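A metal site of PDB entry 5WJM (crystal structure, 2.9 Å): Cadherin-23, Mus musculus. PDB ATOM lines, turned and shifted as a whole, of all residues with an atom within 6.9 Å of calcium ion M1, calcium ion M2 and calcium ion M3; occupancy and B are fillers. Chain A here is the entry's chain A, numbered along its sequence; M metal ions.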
ATOM      1  N   GLU A  19      -6.378  22.570 -20.190  1.00  0.00           N
ATOM      2  CA  GLU A  19      -5.539  23.343 -21.100  1.00  0.00           C
ATOM      3  C   GLU A  19      -6.205  24.695 -21.401  1.00  0.00           C
ATOM      4  O   GLU A  19      -7.419  24.842 -21.290  1.00  0.00           O
ATOM      5  CB  GLU A  19      -5.205  22.564 -22.402  1.00  0.00           C
ATOM      6  CG  GLU A  19      -6.383  22.204 -23.313  1.00  0.00           C
ATOM      7  CD  GLU A  19      -5.997  21.753 -24.734  1.00  0.00           C
ATOM      8  OE1 GLU A  19      -4.909  22.046 -25.264  1.00  0.00           O
ATOM      9  OE2 GLU A  19      -6.828  21.077 -25.364  1.00  0.00           O
ATOM     10  N   GLY A  20      -5.380  25.681 -21.746  1.00  0.00           N
ATOM     11  CA  GLY A  20      -5.878  27.019 -22.153  1.00  0.00           C
ATOM     12  C   GLY A  20      -6.232  27.944 -20.998  1.00  0.00           C
ATOM     13  O   GLY A  20      -6.710  29.061 -21.215  1.00  0.00           O
ATOM     14  N   LEU A  72      -1.423  25.657 -20.018  1.00  0.00           N
ATOM     15  CA  LEU A  72      -1.024  24.314 -20.455  1.00  0.00           C
ATOM     16  C   LEU A  72      -1.654  23.966 -21.837  1.00  0.00           C
ATOM     17  O   LEU A  72      -2.605  24.613 -22.259  1.00  0.00           O
ATOM     18  CB  LEU A  72      -1.393  23.266 -19.400  1.00  0.00           C
ATOM     19  CG  LEU A  72      -0.787  23.401 -18.002  1.00  0.00           C
ATOM     20  CD1 LEU A  72      -1.269  22.288 -17.097  1.00  0.00           C
ATOM     21  CD2 LEU A  72       0.723  23.353 -18.029  1.00  0.00           C
ATOM     22  N   ASP A  73      -1.092  22.949 -22.507  1.00  0.00           N
ATOM     23  CA  ASP A  73      -1.541  22.466 -23.834  1.00  0.00           C
ATOM     24  C   ASP A  73      -1.450  20.927 -23.921  1.00  0.00           C
ATOM     25  O   ASP A  73      -0.373  20.362 -24.011  1.00  0.00           O
ATOM     26  CB  ASP A  73      -0.696  23.126 -24.930  1.00  0.00           C
ATOM     27  CG  ASP A  73      -0.939  22.518 -26.347  1.00  0.00           C
ATOM     28  OD1 ASP A  73      -2.113  22.195 -26.704  1.00  0.00           O
ATOM     29  OD2 ASP A  73       0.049  22.379 -27.120  1.00  0.00           O
ATOM     30  N   ARG A  74      -2.600  20.265 -23.930  1.00  0.00           N
ATOM     31  CA  ARG A  74      -2.669  18.800 -23.960  1.00  0.00           C
ATOM     32  C   ARG A  74      -2.016  18.139 -25.170  1.00  0.00           C
ATOM     33  O   ARG A  74      -1.499  17.008 -25.092  1.00  0.00           O
ATOM     34  CB  ARG A  74      -4.114  18.363 -23.904  1.00  0.00           C
ATOM     35  CG  ARG A  74      -4.289  16.926 -23.472  1.00  0.00           C
ATOM     36  CD  ARG A  74      -5.709  16.490 -23.717  1.00  0.00           C
ATOM     37  NE  ARG A  74      -5.949  16.499 -25.162  1.00  0.00           N
ATOM     38  CZ  ARG A  74      -5.655  15.511 -26.002  1.00  0.00           C
ATOM     39  NH1 ARG A  74      -5.155  14.361 -25.565  1.00  0.00           N
ATOM     40  NH2 ARG A  74      -5.892  15.658 -27.288  1.00  0.00           N
ATOM     41  N   GLU A  75      -2.066  18.818 -26.317  1.00  0.00           N
ATOM     42  CA  GLU A  75      -1.487  18.283 -27.560  1.00  0.00           C
ATOM     43  C   GLU A  75       0.081  18.263 -27.590  1.00  0.00           C
ATOM     44  O   GLU A  75       0.665  17.546 -28.426  1.00  0.00           O
ATOM     45  CB  GLU A  75      -2.034  19.050 -28.781  1.00  0.00           C
ATOM     46  CG  GLU A  75      -3.493  18.754 -29.131  1.00  0.00           C
ATOM     47  CD  GLU A  75      -4.538  19.463 -28.255  1.00  0.00           C
ATOM     48  OE1 GLU A  75      -5.477  18.765 -27.804  1.00  0.00           O
ATOM     49  OE2 GLU A  75      -4.481  20.704 -28.037  1.00  0.00           O
ATOM     50  N   THR A  76       0.768  19.042 -26.700  1.00  0.00           N
ATOM     51  CA  THR A  76       2.229  18.935 -26.548  1.00  0.00           C
ATOM     52  C   THR A  76       2.575  18.105 -25.308  1.00  0.00           C
ATOM     53  O   THR A  76       3.432  17.227 -25.373  1.00  0.00           O
ATOM     54  CB  THR A  76       2.977  20.298 -26.579  1.00  0.00           C
ATOM     55  OG1 THR A  76       2.452  21.164 -25.602  1.00  0.00           O
ATOM     56  CG2 THR A  76       2.865  21.004 -27.959  1.00  0.00           C
ATOM     57  N   LEU A 105      -6.530  18.139 -18.856  1.00  0.00           N
ATOM     58  CA  LEU A 105      -7.863  17.933 -19.439  1.00  0.00           C
ATOM     59  C   LEU A 105      -8.014  18.710 -20.749  1.00  0.00           C
ATOM     60  O   LEU A 105      -7.633  19.890 -20.837  1.00  0.00           O
ATOM     61  CB  LEU A 105      -8.981  18.381 -18.496  1.00  0.00           C
ATOM     62  CG  LEU A 105      -9.246  17.654 -17.167  1.00  0.00           C
ATOM     63  CD1 LEU A 105     -10.333  18.429 -16.407  1.00  0.00           C
ATOM     64  CD2 LEU A 105      -9.625  16.188 -17.322  1.00  0.00           C
ATOM     65  N   ASP A 106      -8.612  18.044 -21.736  1.00  0.00           N
ATOM     66  CA  ASP A 106      -8.706  18.535 -23.116  1.00  0.00           C
ATOM     67  C   ASP A 106      -9.755  19.622 -23.275  1.00  0.00           C
ATOM     68  O   ASP A 106     -10.803  19.512 -22.699  1.00  0.00           O
ATOM     69  CB  ASP A 106      -9.111  17.361 -24.003  1.00  0.00           C
ATOM     70  CG  ASP A 106      -9.149  17.714 -25.453  1.00  0.00           C
ATOM     71  OD1 ASP A 106      -8.164  18.295 -25.949  1.00  0.00           O
ATOM     72  OD2 ASP A 106     -10.144  17.374 -26.121  1.00  0.00           O
ATOM     73  N   ILE A 107      -9.480  20.654 -24.073  1.00  0.00           N
ATOM     74  CA  ILE A 107     -10.560  21.503 -24.607  1.00  0.00           C
ATOM     75  C   ILE A 107     -10.607  21.291 -26.117  1.00  0.00           C
ATOM     76  O   ILE A 107      -9.702  20.646 -26.671  1.00  0.00           O
ATOM     77  CB  ILE A 107     -10.432  23.010 -24.238  1.00  0.00           C
ATOM     78  CG1 ILE A 107      -9.374  23.735 -25.092  1.00  0.00           C
ATOM     79  CG2 ILE A 107     -10.197  23.175 -22.738  1.00  0.00           C
ATOM     80  CD1 ILE A 107      -9.084  25.163 -24.675  1.00  0.00           C
ATOM     81  N   ASN A 108     -11.652  21.816 -26.764  1.00  0.00           N
ATOM     82  CA  ASN A 108     -11.810  21.669 -28.210  1.00  0.00           C
ATOM     83  C   ASN A 108     -11.147  22.839 -28.936  1.00  0.00           C
ATOM     84  O   ASN A 108     -11.773  23.844 -29.271  1.00  0.00           O
ATOM     85  CB  ASN A 108     -13.283  21.541 -28.578  1.00  0.00           C
ATOM     86  CG  ASN A 108     -13.487  21.069 -30.009  1.00  0.00           C
ATOM     87  OD1 ASN A 108     -12.786  20.173 -30.491  1.00  0.00           O
ATOM     88  ND2 ASN A 108     -14.449  21.672 -30.691  1.00  0.00           N
ATOM     89  N   ASP A 109      -9.862  22.696 -29.167  1.00  0.00           N
ATOM     90  CA  ASP A 109      -9.055  23.754 -29.701  1.00  0.00           C
ATOM     91  C   ASP A 109      -8.399  23.339 -31.023  1.00  0.00           C
ATOM     92  O   ASP A 109      -7.416  23.958 -31.457  1.00  0.00           O
ATOM     93  CB  ASP A 109      -8.040  24.249 -28.625  1.00  0.00           C
ATOM     94  CG  ASP A 109      -7.052  23.168 -28.129  1.00  0.00           C
ATOM     95  OD1 ASP A 109      -7.466  22.028 -27.836  1.00  0.00           O
ATOM     96  OD2 ASP A 109      -5.837  23.446 -28.027  1.00  0.00           O
ATOM     97  N   ASN A 110      -8.958  22.309 -31.662  1.00  0.00           N
ATOM     98  CA  ASN A 110      -8.451  21.794 -32.939  1.00  0.00           C
ATOM     99  C   ASN A 110      -9.634  21.452 -33.866  1.00  0.00           C
ATOM    100  O   ASN A 110     -10.508  20.651 -33.505  1.00  0.00           O
ATOM    101  CB  ASN A 110      -7.592  20.543 -32.762  1.00  0.00           C
ATOM    102  CG  ASN A 110      -6.299  20.798 -31.988  1.00  0.00           C
ATOM    103  OD1 ASN A 110      -5.224  20.930 -32.578  1.00  0.00           O
ATOM    104  ND2 ASN A 110      -6.386  20.813 -30.665  1.00  0.00           N
ATOM    105  N   ASP A 111      -9.632  22.056 -35.049  1.00  0.00           N
ATOM    106  CA  ASP A 111     -10.612  21.762 -36.095  1.00  0.00           C
ATOM    107  C   ASP A 111     -10.467  20.314 -36.558  1.00  0.00           C
ATOM    108  O   ASP A 111      -9.353  19.778 -36.579  1.00  0.00           O
ATOM    109  CB  ASP A 111     -10.433  22.719 -37.308  1.00  0.00           C
ATOM    110  CG  ASP A 111     -10.920  24.167 -37.035  1.00  0.00           C
ATOM    111  OD1 ASP A 111     -11.552  24.439 -35.994  1.00  0.00           O
ATOM    112  OD2 ASP A 111     -10.673  25.060 -37.901  1.00  0.00           O
ATOM    113  N   PRO A 112     -11.571  19.650 -36.937  1.00  0.00           N
ATOM    114  CA  PRO A 112     -11.383  18.405 -37.683  1.00  0.00           C
ATOM    115  C   PRO A 112     -10.822  18.721 -39.054  1.00  0.00           C
ATOM    116  O   PRO A 112     -10.942  19.852 -39.500  1.00  0.00           O
ATOM    117  CB  PRO A 112     -12.807  17.809 -37.768  1.00  0.00           C
ATOM    118  CG  PRO A 112     -13.725  18.940 -37.519  1.00  0.00           C
ATOM    119  CD  PRO A 112     -12.993  19.947 -36.689  1.00  0.00           C
ATOM    120  N   ASP A 140      -8.766  14.440 -36.065  1.00  0.00           N
ATOM    121  CA  ASP A 140      -8.932  15.524 -35.062  1.00  0.00           C
ATOM    122  C   ASP A 140      -7.900  15.321 -33.923  1.00  0.00           C
ATOM    123  O   ASP A 140      -7.814  14.252 -33.309  1.00  0.00           O
ATOM    124  CB  ASP A 140     -10.370  15.548 -34.531  1.00  0.00           C
ATOM    125  CG  ASP A 140     -10.752  16.872 -33.826  1.00  0.00           C
ATOM    126  OD1 ASP A 140     -10.137  17.238 -32.794  1.00  0.00           O
ATOM    127  OD2 ASP A 140     -11.705  17.543 -34.276  1.00  0.00           O
ATOM    128  N   ALA A 141      -7.128  16.351 -33.659  1.00  0.00           N
ATOM    129  CA  ALA A 141      -6.011  16.266 -32.723  1.00  0.00           C
ATOM    130  C   ALA A 141      -6.436  16.200 -31.242  1.00  0.00           C
ATOM    131  O   ALA A 141      -5.635  15.809 -30.385  1.00  0.00           O
ATOM    132  CB  ALA A 141      -5.044  17.428 -32.957  1.00  0.00           C
ATOM    133  N   ASP A 142      -7.693  16.585 -30.952  1.00  0.00           N
ATOM    134  CA  ASP A 142      -8.247  16.562 -29.590  1.00  0.00           C
ATOM    135  C   ASP A 142      -8.480  15.100 -29.147  1.00  0.00           C
ATOM    136  O   ASP A 142      -8.131  14.159 -29.879  1.00  0.00           O
ATOM    137  CB  ASP A 142      -9.535  17.409 -29.507  1.00  0.00           C
ATOM    138  CG  ASP A 142      -9.299  18.921 -29.838  1.00  0.00           C
ATOM    139  OD1 ASP A 142      -8.340  19.539 -29.315  1.00  0.00           O
ATOM    140  OD2 ASP A 142     -10.081  19.502 -30.643  1.00  0.00           O
ATOM    141  N   SER A 143      -9.009  14.922 -27.947  1.00  0.00           N
ATOM    142  CA  SER A 143      -9.360  13.606 -27.421  1.00  0.00           C
ATOM    143  C   SER A 143     -10.826  13.575 -27.043  1.00  0.00           C
ATOM    144  O   SER A 143     -11.502  14.619 -27.071  1.00  0.00           O
ATOM    145  CB  SER A 143      -8.510  13.278 -26.191  1.00  0.00           C
ATOM    146  OG  SER A 143      -9.074  13.884 -25.029  1.00  0.00           O
ATOM    147  N   CYS A 145     -14.822  13.268 -26.657  1.00  0.00           N
ATOM    148  CA  CYS A 145     -15.921  13.805 -27.469  1.00  0.00           C
ATOM    149  C   CYS A 145     -15.468  14.964 -28.390  1.00  0.00           C
ATOM    150  O   CYS A 145     -16.107  15.263 -29.414  1.00  0.00           O
ATOM    151  CB  CYS A 145     -17.086  14.242 -26.569  1.00  0.00           C
ATOM    152  SG  CYS A 145     -16.819  15.728 -25.585  1.00  0.00           S
ATOM    153  N   ASN A 146     -14.340  15.609 -28.056  1.00  0.00           N
ATOM    154  CA  ASN A 146     -13.780  16.703 -28.885  1.00  0.00           C
ATOM    155  C   ASN A 146     -13.107  16.238 -30.180  1.00  0.00           C
ATOM    156  O   ASN A 146     -12.721  17.076 -31.007  1.00  0.00           O
ATOM    157  CB  ASN A 146     -12.762  17.531 -28.070  1.00  0.00           C
ATOM    158  CG  ASN A 146     -13.384  18.196 -26.858  1.00  0.00           C
ATOM    159  OD1 ASN A 146     -14.544  18.575 -26.869  1.00  0.00           O
ATOM    160  ND2 ASN A 146     -12.606  18.359 -25.805  1.00  0.00           N
ATOM    161  N   ALA A 147     -12.909  14.934 -30.324  1.00  0.00           N
ATOM    162  CA  ALA A 147     -12.422  14.346 -31.572  1.00  0.00           C
ATOM    163  C   ALA A 147     -13.363  13.268 -32.131  1.00  0.00           C
ATOM    164  O   ALA A 147     -13.004  12.576 -33.079  1.00  0.00           O
ATOM    165  CB  ALA A 147     -11.016  13.786 -31.380  1.00  0.00           C
ATOM    166  N   LEU A 148     -14.580  13.169 -31.585  1.00  0.00           N
ATOM    167  CA  LEU A 148     -15.590  12.244 -32.110  1.00  0.00           C
ATOM    168  C   LEU A 148     -16.262  12.935 -33.290  1.00  0.00           C
ATOM    169  O   LEU A 148     -16.957  13.944 -33.100  1.00  0.00           O
ATOM    170  CB  LEU A 148     -16.637  11.904 -31.030  1.00  0.00           C
ATOM    171  CG  LEU A 148     -17.871  11.113 -31.532  1.00  0.00           C
ATOM    172  CD1 LEU A 148     -17.443   9.783 -32.136  1.00  0.00           C
ATOM    173  CD2 LEU A 148     -18.915  10.904 -30.436  1.00  0.00           C
ATOM    174  N   LEU A 149     -16.069  12.392 -34.506  1.00  0.00           N
ATOM    175  CA  LEU A 149     -16.487  13.072 -35.741  1.00  0.00           C
ATOM    176  C   LEU A 149     -17.806  12.564 -36.331  1.00  0.00           C
ATOM    177  O   LEU A 149     -18.076  11.356 -36.328  1.00  0.00           O
ATOM    178  CB  LEU A 149     -15.379  12.960 -36.791  1.00  0.00           C
ATOM    179  CG  LEU A 149     -14.006  13.453 -36.369  1.00  0.00           C
ATOM    180  CD1 LEU A 149     -13.060  13.462 -37.553  1.00  0.00           C
ATOM    181  CD2 LEU A 149     -14.099  14.826 -35.744  1.00  0.00           C
ATOM    182  N   ASP A 193     -16.825  17.915 -35.162  1.00  0.00           N
ATOM    183  CA  ASP A 193     -16.659  17.258 -33.864  1.00  0.00           C
ATOM    184  C   ASP A 193     -17.909  17.507 -32.991  1.00  0.00           C
ATOM    185  O   ASP A 193     -18.805  18.274 -33.348  1.00  0.00           O
ATOM    186  CB  ASP A 193     -15.322  17.595 -33.140  1.00  0.00           C
ATOM    187  CG  ASP A 193     -15.014  19.097 -33.076  1.00  0.00           C
ATOM    188  OD1 ASP A 193     -15.948  19.914 -32.991  1.00  0.00           O
ATOM    189  OD2 ASP A 193     -13.824  19.464 -33.105  1.00  0.00           O
ATOM    190  N   ASN A 194     -17.952  16.802 -31.867  1.00  0.00           N
ATOM    191  CA  ASN A 194     -19.142  16.766 -31.012  1.00  0.00           C
ATOM    192  C   ASN A 194     -18.742  16.994 -29.566  1.00  0.00           C
ATOM    193  O   ASN A 194     -18.840  16.084 -28.754  1.00  0.00           O
ATOM    194  CB  ASN A 194     -19.860  15.412 -31.168  1.00  0.00           C
ATOM    195  CG  ASN A 194     -20.359  15.186 -32.573  1.00  0.00           C
ATOM    196  OD1 ASN A 194     -21.505  15.464 -32.878  1.00  0.00           O
ATOM    197  ND2 ASN A 194     -19.487  14.699 -33.446  1.00  0.00           N
ATOM    198  N   PRO A 195     -18.304  18.220 -29.223  1.00  0.00           N
ATOM    199  CA  PRO A 195     -17.973  18.523 -27.836  1.00  0.00           C
ATOM    200  C   PRO A 195     -19.219  18.525 -26.966  1.00  0.00           C
ATOM    201  O   PRO A 195     -20.315  18.562 -27.501  1.00  0.00           O
ATOM    202  CB  PRO A 195     -17.344  19.923 -27.910  1.00  0.00           C
ATOM    203  CG  PRO A 195     -17.816  20.509 -29.187  1.00  0.00           C
ATOM    204  CD  PRO A 195     -18.153  19.381 -30.122  1.00  0.00           C
ATOM    205  N   ARG A 202     -16.419  22.514 -33.898  1.00  0.00           N
ATOM    206  CA  ARG A 202     -15.628  22.959 -35.054  1.00  0.00           C
ATOM    207  C   ARG A 202     -15.852  22.005 -36.236  1.00  0.00           C
ATOM    208  O   ARG A 202     -16.177  20.832 -36.029  1.00  0.00           O
ATOM    209  CB  ARG A 202     -14.157  23.040 -34.662  1.00  0.00           C
ATOM    210  CG  ARG A 202     -13.908  23.723 -33.317  1.00  0.00           C
ATOM    211  CD  ARG A 202     -12.548  23.409 -32.710  1.00  0.00           C
ATOM    212  NE  ARG A 202     -11.575  24.436 -33.094  1.00  0.00           N
ATOM    213  CZ  ARG A 202     -11.333  25.561 -32.418  1.00  0.00           C
ATOM    214  NH1 ARG A 202     -11.961  25.828 -31.271  1.00  0.00           N
ATOM    215  NH2 ARG A 202     -10.440  26.425 -32.889  1.00  0.00           N
HETATM  216 CA    CA M   1      -4.035  22.853 -27.234  1.00  0.00          CA
HETATM  217 CA    CA M   2      -7.422  19.869 -27.210  1.00  0.00          CA
HETATM  218 CA    CA M   3     -11.661  18.959 -32.136  1.00  0.00          CA
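The side-chain carboxylate (OD2) of Asp 73 lies within hydrogen-bond range of the side-chain hydroxyl (OG1) of Thr 76 (3.1 Å). The side-chain amide nitrogen (ND2) of Asn 146 is in hydrogen-bond range of the side-chain carboxylate (OD2) of Asp 106. The side-chain carboxylate (OD1) of Asp 106 sits close to the guanidinium group (NE) of Arg 74 (3.0 Å). The backbone NH of Ser 143 sits at hydrogen-bond distance from the side-chain carboxylate of Asp 106 (3.3 Å). OE1 of Glu 19 sits close to N of Arg 74 (3.2 Å). The backbone NH of Glu 19 sits at hydrogen-bond distance from the backbone carbonyl oxygen of Leu 105 (3.0 Å). OE2 of Glu 75 lies close to ND2 of Asn 110 (3.2 Å). The guanidinium group of Arg 74 lies close to the side-chain carboxylate of Glu 75 (3.2 Å).
Within 4 Å of calcium ion M1: Glu 19, Asp 73, Glu 75 and Asp 109. The nearest printed residue that does not touch calcium ion M1 is Arg 74 (4.4 Å).
Seven residues have an atom within 4 Å of calcium ion M2: Glu 19, Glu 75, Asp 106, Ile 107, Asp 109, Asn 110 and Asp 142.
Of the 28 residues printed, 6 come within 4 Å of calcium ion M3.
Calcium ion M1 is bound by OD2 of Asp 109 (2.1 Å), OD1 of Asp 73 (2.1 Å), OE1 of Glu 19 (2.3 Å) and OE2 of Glu 75 (2.3 Å). Calcium ion M1 has four donor atoms within binding distance.
The side-chain carboxylate (OD1) of Asp 106 is bound to calcium ion M2 (2.1 Å). OD1 of Asp 109 binds calcium ion M2 (2.2 Å). OE2 of Glu 19 is bound to calcium ion M2 (2.3 Å). The side-chain carboxylate (OE1) of Glu 75 is bound to calcium ion M2. OD1 of Asp 142 binds calcium ion M2, 2.3 Å away. O of Ile 107 binds calcium ion M2.
Calcium ion M3 is bound by the side-chain carboxylate (OD2) of Asp 142, the side-chain amide oxygen (OD1) of Asn 108, the side-chain carboxylate (OD1) of Asp 140, the side-chain carboxylate (OD2) of Asp 193, the backbone carbonyl oxygen (O) of Asn 146, the backbone carbonyl oxygen (O) of Asn 110 and the side-chain carboxylate (OD2) of Asp 140.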
